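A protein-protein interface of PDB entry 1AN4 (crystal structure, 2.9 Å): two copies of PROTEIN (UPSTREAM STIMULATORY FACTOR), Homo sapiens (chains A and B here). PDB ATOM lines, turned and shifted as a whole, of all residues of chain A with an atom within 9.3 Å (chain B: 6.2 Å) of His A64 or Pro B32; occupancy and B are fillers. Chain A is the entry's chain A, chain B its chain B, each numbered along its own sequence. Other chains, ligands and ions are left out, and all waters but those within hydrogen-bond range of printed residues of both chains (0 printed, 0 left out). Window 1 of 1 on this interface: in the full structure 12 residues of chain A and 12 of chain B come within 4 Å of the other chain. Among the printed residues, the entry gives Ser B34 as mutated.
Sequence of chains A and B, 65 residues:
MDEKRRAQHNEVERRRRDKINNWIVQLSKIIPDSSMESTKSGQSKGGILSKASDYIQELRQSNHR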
ATOM      1  N   ILE A  56     -20.587  25.427  34.108  1.00  0.00           N
ATOM      2  CA  ILE A  56     -20.595  24.994  32.715  1.00  0.00           C
ATOM      3  C   ILE A  56     -21.992  24.739  32.131  1.00  0.00           C
ATOM      4  O   ILE A  56     -22.259  25.053  30.976  1.00  0.00           O
ATOM      5  CB  ILE A  56     -19.703  23.751  32.509  1.00  0.00           C
ATOM      6  CG1 ILE A  56     -18.279  24.032  33.008  1.00  0.00           C
ATOM      7  CG2 ILE A  56     -19.658  23.379  31.025  1.00  0.00           C
ATOM      8  CD1 ILE A  56     -18.057  23.684  34.423  1.00  0.00           C
ATOM      9  N   GLN A  57     -22.898  24.170  32.908  1.00  0.00           N
ATOM     10  CA  GLN A  57     -24.222  23.941  32.367  1.00  0.00           C
ATOM     11  C   GLN A  57     -24.836  25.326  32.173  1.00  0.00           C
ATOM     12  O   GLN A  57     -25.049  25.760  31.028  1.00  0.00           O
ATOM     13  CB  GLN A  57     -25.058  23.028  33.297  1.00  0.00           C
ATOM     14  CG  GLN A  57     -25.912  23.701  34.354  1.00  0.00           C
ATOM     15  CD  GLN A  57     -27.373  23.825  33.935  1.00  0.00           C
ATOM     16  OE1 GLN A  57     -28.035  22.820  33.667  1.00  0.00           O
ATOM     17  NE2 GLN A  57     -27.879  25.056  33.883  1.00  0.00           N
ATOM     18  N   GLU A  58     -24.907  26.080  33.276  1.00  0.00           N
ATOM     19  CA  GLU A  58     -25.472  27.413  33.283  1.00  0.00           C
ATOM     20  C   GLU A  58     -24.616  28.411  32.525  1.00  0.00           C
ATOM     21  O   GLU A  58     -24.734  29.598  32.775  1.00  0.00           O
ATOM     22  CB  GLU A  58     -25.712  27.918  34.722  1.00  0.00           C
ATOM     23  CG  GLU A  58     -24.489  28.516  35.503  1.00  0.00           C
ATOM     24  CD  GLU A  58     -24.895  29.447  36.698  1.00  0.00           C
ATOM     25  OE1 GLU A  58     -25.977  30.093  36.610  1.00  0.00           O
ATOM     26  OE2 GLU A  58     -24.133  29.549  37.709  1.00  0.00           O
ATOM     27  N   LEU A  59     -23.715  27.952  31.657  1.00  0.00           N
ATOM     28  CA  LEU A  59     -22.907  28.856  30.875  1.00  0.00           C
ATOM     29  C   LEU A  59     -23.150  28.509  29.411  1.00  0.00           C
ATOM     30  O   LEU A  59     -23.182  29.396  28.524  1.00  0.00           O
ATOM     31  CB  LEU A  59     -21.448  28.737  31.267  1.00  0.00           C
ATOM     32  CG  LEU A  59     -20.816  29.606  32.392  1.00  0.00           C
ATOM     33  CD1 LEU A  59     -19.985  30.791  31.825  1.00  0.00           C
ATOM     34  CD2 LEU A  59     -21.831  30.066  33.461  1.00  0.00           C
ATOM     35  N   ARG A  60     -23.374  27.221  29.148  1.00  0.00           N
ATOM     36  CA  ARG A  60     -23.695  26.765  27.782  1.00  0.00           C
ATOM     37  C   ARG A  60     -25.120  27.220  27.567  1.00  0.00           C
ATOM     38  O   ARG A  60     -25.414  28.048  26.696  1.00  0.00           O
ATOM     39  CB  ARG A  60     -23.692  25.232  27.673  1.00  0.00           C
ATOM     40  CG  ARG A  60     -24.073  24.683  26.282  1.00  0.00           C
ATOM     41  CD  ARG A  60     -25.585  24.566  26.034  1.00  0.00           C
ATOM     42  NE  ARG A  60     -26.202  23.390  26.658  1.00  0.00           N
ATOM     43  CZ  ARG A  60     -26.680  22.346  25.976  1.00  0.00           C
ATOM     44  NH1 ARG A  60     -26.599  22.322  24.646  1.00  0.00           N
ATOM     45  NH2 ARG A  60     -27.283  21.341  26.617  1.00  0.00           N
ATOM     46  N   GLN A  61     -25.980  26.645  28.407  1.00  0.00           N
ATOM     47  CA  GLN A  61     -27.414  26.889  28.451  1.00  0.00           C
ATOM     48  C   GLN A  61     -27.732  28.303  27.936  1.00  0.00           C
ATOM     49  O   GLN A  61     -27.883  28.507  26.724  1.00  0.00           O
ATOM     50  CB  GLN A  61     -27.881  26.677  29.915  1.00  0.00           C
ATOM     51  CG  GLN A  61     -29.385  26.747  30.237  1.00  0.00           C
ATOM     52  CD  GLN A  61     -29.682  27.680  31.429  1.00  0.00           C
ATOM     53  OE1 GLN A  61     -29.124  27.520  32.516  1.00  0.00           O
ATOM     54  NE2 GLN A  61     -30.534  28.674  31.205  1.00  0.00           N
ATOM     55  N   SER A  62     -27.661  29.276  28.838  1.00  0.00           N
ATOM     56  CA  SER A  62     -27.984  30.661  28.555  1.00  0.00           C
ATOM     57  C   SER A  62     -27.247  31.379  27.432  1.00  0.00           C
ATOM     58  O   SER A  62     -27.653  32.491  27.110  1.00  0.00           O
ATOM     59  CB  SER A  62     -27.788  31.490  29.822  1.00  0.00           C
ATOM     60  OG  SER A  62     -27.928  30.694  30.981  1.00  0.00           O
ATOM     61  N   ASN A  63     -26.210  30.804  26.809  1.00  0.00           N
ATOM     62  CA  ASN A  63     -25.486  31.583  25.787  1.00  0.00           C
ATOM     63  C   ASN A  63     -24.771  30.935  24.561  1.00  0.00           C
ATOM     64  O   ASN A  63     -24.910  31.436  23.446  1.00  0.00           O
ATOM     65  CB  ASN A  63     -24.501  32.533  26.506  1.00  0.00           C
ATOM     66  CG  ASN A  63     -25.202  33.521  27.459  1.00  0.00           C
ATOM     67  OD1 ASN A  63     -25.034  33.483  28.694  1.00  0.00           O
ATOM     68  ND2 ASN A  63     -26.023  34.389  26.885  1.00  0.00           N
ATOM     69  N   HIS A  64     -23.969  29.884  24.778  1.00  0.00           N
ATOM     70  CA  HIS A  64     -23.180  29.175  23.733  1.00  0.00           C
ATOM     71  C   HIS A  64     -24.025  28.164  22.921  1.00  0.00           C
ATOM     72  O   HIS A  64     -24.792  27.402  23.513  1.00  0.00           O
ATOM     73  CB  HIS A  64     -21.948  28.513  24.426  1.00  0.00           C
ATOM     74  CG  HIS A  64     -21.213  27.474  23.613  1.00  0.00           C
ATOM     75  ND1 HIS A  64     -20.340  26.576  24.194  1.00  0.00           N
ATOM     76  CD2 HIS A  64     -21.215  27.187  22.285  1.00  0.00           C
ATOM     77  CE1 HIS A  64     -19.838  25.782  23.261  1.00  0.00           C
ATOM     78  NE2 HIS A  64     -20.354  26.130  22.094  1.00  0.00           N
ATOM     79  N   ARG A  65     -23.837  28.156  21.588  1.00  0.00           N
ATOM     80  CA  ARG A  65     -24.549  27.290  20.631  1.00  0.00           C
ATOM     81  C   ARG A  65     -26.017  27.128  20.972  1.00  0.00           C
ATOM     82  O   ARG A  65     -26.337  26.344  21.885  1.00  0.00           O
ATOM     83  CB  ARG A  65     -23.911  25.910  20.498  1.00  0.00           C
ATOM     84  CG  ARG A  65     -23.356  25.629  19.094  1.00  0.00           C
ATOM     85  CD  ARG A  65     -23.464  24.134  18.633  1.00  0.00           C
ATOM     86  NE  ARG A  65     -22.205  23.515  18.176  1.00  0.00           N
ATOM     87  CZ  ARG A  65     -21.634  22.481  18.793  1.00  0.00           C
ATOM     88  NH1 ARG A  65     -22.192  21.974  19.871  1.00  0.00           N
ATOM     89  NH2 ARG A  65     -20.540  21.914  18.318  1.00  0.00           N
ATOM     90  N   LYS B  29     -20.998  16.697  27.647  1.00  0.00           N
ATOM     91  CA  LYS B  29     -21.777  16.569  26.414  1.00  0.00           C
ATOM     92  C   LYS B  29     -22.468  17.852  25.953  1.00  0.00           C
ATOM     93  O   LYS B  29     -22.576  18.062  24.748  1.00  0.00           O
ATOM     94  CB  LYS B  29     -22.817  15.437  26.530  1.00  0.00           C
ATOM     95  CG  LYS B  29     -23.121  14.662  25.224  1.00  0.00           C
ATOM     96  CD  LYS B  29     -24.044  13.455  25.493  1.00  0.00           C
ATOM     97  CE  LYS B  29     -23.430  12.512  26.549  1.00  0.00           C
ATOM     98  NZ  LYS B  29     -24.165  11.269  27.065  1.00  0.00           N
ATOM     99  N   ILE B  30     -22.902  18.719  26.877  1.00  0.00           N
ATOM    100  CA  ILE B  30     -23.583  19.962  26.475  1.00  0.00           C
ATOM    101  C   ILE B  30     -22.697  20.869  25.633  1.00  0.00           C
ATOM    102  O   ILE B  30     -23.172  21.735  24.890  1.00  0.00           O
ATOM    103  CB  ILE B  30     -24.260  20.745  27.667  1.00  0.00           C
ATOM    104  CG1 ILE B  30     -23.273  21.630  28.445  1.00  0.00           C
ATOM    105  CG2 ILE B  30     -25.021  19.769  28.585  1.00  0.00           C
ATOM    106  CD1 ILE B  30     -23.978  22.544  29.504  1.00  0.00           C
ATOM    107  N   ILE B  31     -21.402  20.628  25.734  1.00  0.00           N
ATOM    108  CA  ILE B  31     -20.411  21.348  24.947  1.00  0.00           C
ATOM    109  C   ILE B  31     -20.179  20.492  23.655  1.00  0.00           C
ATOM    110  O   ILE B  31     -20.103  19.248  23.735  1.00  0.00           O
ATOM    111  CB  ILE B  31     -19.112  21.572  25.764  1.00  0.00           C
ATOM    112  CG1 ILE B  31     -19.082  20.647  26.977  1.00  0.00           C
ATOM    113  CG2 ILE B  31     -18.992  23.022  26.164  1.00  0.00           C
ATOM    114  CD1 ILE B  31     -18.921  19.180  26.617  1.00  0.00           C
ATOM    115  N   PRO B  32     -19.930  21.158  22.490  1.00  0.00           N
ATOM    116  CA  PRO B  32     -19.685  20.729  21.094  1.00  0.00           C
ATOM    117  C   PRO B  32     -20.049  19.360  20.583  1.00  0.00           C
ATOM    118  O   PRO B  32     -19.573  18.337  21.081  1.00  0.00           O
ATOM    119  CB  PRO B  32     -18.197  21.037  20.868  1.00  0.00           C
ATOM    120  CG  PRO B  32     -17.747  21.573  22.185  1.00  0.00           C
ATOM    121  CD  PRO B  32     -18.971  22.236  22.739  1.00  0.00           C
ATOM    122  N   ASP B  33     -20.831  19.377  19.512  1.00  0.00           N
ATOM    123  CA  ASP B  33     -21.272  18.161  18.871  1.00  0.00           C
ATOM    124  C   ASP B  33     -20.094  17.284  18.428  1.00  0.00           C
ATOM    125  O   ASP B  33     -19.424  17.506  17.407  1.00  0.00           O
ATOM    126  CB  ASP B  33     -22.262  18.466  17.749  1.00  0.00           C
ATOM    127  CG  ASP B  33     -23.575  19.030  18.280  1.00  0.00           C
ATOM    128  OD1 ASP B  33     -23.989  18.623  19.396  1.00  0.00           O
ATOM    129  OD2 ASP B  33     -24.189  19.885  17.591  1.00  0.00           O
ATOM    130  N   SER B  34     -19.800  16.358  19.332  1.00  0.00           N
ATOM    131  CA  SER B  34     -18.745  15.373  19.236  1.00  0.00           C
ATOM    132  C   SER B  34     -19.145  14.247  18.303  1.00  0.00           C
ATOM    133  O   SER B  34     -19.507  14.486  17.155  1.00  0.00           O
ATOM    134  CB  SER B  34     -18.545  14.812  20.628  1.00  0.00           C
ATOM    135  OG  SER B  34     -19.821  14.391  21.060  1.00  0.00           O
ATOM    136  N   SER B  35     -19.237  13.057  18.897  1.00  0.00           N
ATOM    137  CA  SER B  35     -19.527  11.773  18.265  1.00  0.00           C
ATOM    138  C   SER B  35     -18.164  11.058  17.999  1.00  0.00           C
ATOM    139  O   SER B  35     -17.331  11.464  17.157  1.00  0.00           O
ATOM    140  CB  SER B  35     -20.398  11.917  17.007  1.00  0.00           C
ATOM    141  OG  SER B  35     -21.144  10.734  16.786  1.00  0.00           O
ATOM    142  N   LYS B  51     -11.504  20.221  24.714  1.00  0.00           N
ATOM    143  CA  LYS B  51     -12.256  21.172  23.859  1.00  0.00           C
ATOM    144  C   LYS B  51     -13.119  22.114  24.682  1.00  0.00           C
ATOM    145  O   LYS B  51     -13.468  23.203  24.232  1.00  0.00           O
ATOM    146  CB  LYS B  51     -13.151  20.425  22.848  1.00  0.00           C
ATOM    147  CG  LYS B  51     -12.422  19.476  21.860  1.00  0.00           C
ATOM    148  CD  LYS B  51     -11.335  20.167  20.991  1.00  0.00           C
ATOM    149  CE  LYS B  51      -9.928  20.059  21.615  1.00  0.00           C
ATOM    150  NZ  LYS B  51      -9.445  21.368  22.182  1.00  0.00           N
ATOM    151  N   ALA B  52     -13.480  21.631  25.873  1.00  0.00           N
ATOM    152  CA  ALA B  52     -14.269  22.325  26.889  1.00  0.00           C
ATOM    153  C   ALA B  52     -13.282  23.021  27.820  1.00  0.00           C
ATOM    154  O   ALA B  52     -13.531  23.198  29.027  1.00  0.00           O
ATOM    155  CB  ALA B  52     -15.051  21.337  27.672  1.00  0.00           C
ATOM    156  N   TYR B  55     -13.597  26.688  25.378  1.00  0.00           N
ATOM    157  CA  TYR B  55     -14.902  27.330  25.453  1.00  0.00           C
ATOM    158  C   TYR B  55     -14.927  27.768  26.906  1.00  0.00           C
ATOM    159  O   TYR B  55     -15.439  28.818  27.270  1.00  0.00           O
ATOM    160  CB  TYR B  55     -15.961  26.291  25.118  1.00  0.00           C
ATOM    161  CG  TYR B  55     -15.572  25.493  23.880  1.00  0.00           C
ATOM    162  CD1 TYR B  55     -14.718  26.043  22.894  1.00  0.00           C
ATOM    163  CD2 TYR B  55     -16.112  24.245  23.642  1.00  0.00           C
ATOM    164  CE1 TYR B  55     -14.445  25.374  21.685  1.00  0.00           C
ATOM    165  CE2 TYR B  55     -15.837  23.571  22.453  1.00  0.00           C
ATOM    166  CZ  TYR B  55     -15.026  24.125  21.462  1.00  0.00           C
ATOM    167  OH  TYR B  55     -14.931  23.458  20.237  1.00  0.00           O
ATOM    168  N   LEU B  59     -15.932  31.638  27.503  1.00  0.00           N
ATOM    169  CA  LEU B  59     -17.026  32.097  28.333  1.00  0.00           C
ATOM    170  C   LEU B  59     -16.679  32.015  29.829  1.00  0.00           C
ATOM    171  O   LEU B  59     -17.556  31.822  30.683  1.00  0.00           O
ATOM    172  CB  LEU B  59     -18.293  31.334  27.949  1.00  0.00           C
ATOM    173  CG  LEU B  59     -19.645  31.322  28.673  1.00  0.00           C
ATOM    174  CD1 LEU B  59     -20.053  32.710  29.170  1.00  0.00           C
ATOM    175  CD2 LEU B  59     -20.692  30.689  27.722  1.00  0.00           C
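OE1 of Gln A61 is in hydrogen-bond range of NE2 of Gln A57 (3.1 Å).
Leu B59 touches its own counterpart, Leu A59.
NH1 of Arg A60 lies close to O of Ile B30, at 3.5 Å. The guanidinium group of Arg A65 is in salt-bridge range of the side-chain carboxylate of Asp B33.
Of chain B, only Pro B32 (3.7 Å) comes within 4 Å of His A64. Of chain A, only His A64 and Arg A65 come within 4 Å of Pro B32. Printed residues of chain B within 4 Å of Leu A59: Leu B59. Of the printed residues of chain A, Leu B59 touches Leu A59 (2.9 Å). Of the printed residues of chain A, Ile B30 touches Ile A56, Gln A57 and Arg A60. Of the printed residues of chain B, Arg A65 touches Pro B32 and Asp B33. Ala B52 touches none of the printed residues of chain A. Tyr B55 touches none of the printed residues of chain A. The nearest residue of chain A that does not touch Pro B32 is Arg A60 (6.6 Å).
Among the printed residues, Asp or Glu carboxylates within 4 Å of a Lys or Arg side-chain nitrogen of the other chain: Arg A65 with Asp B33 (3.7 Å).
Among the printed residues, merely in contact across the chains: Leu A59 with Leu B59, Arg A65 with Pro B32, Gln A57 with Ile B30, Ile A56 with Ile B30 and His A64 with Pro B32.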
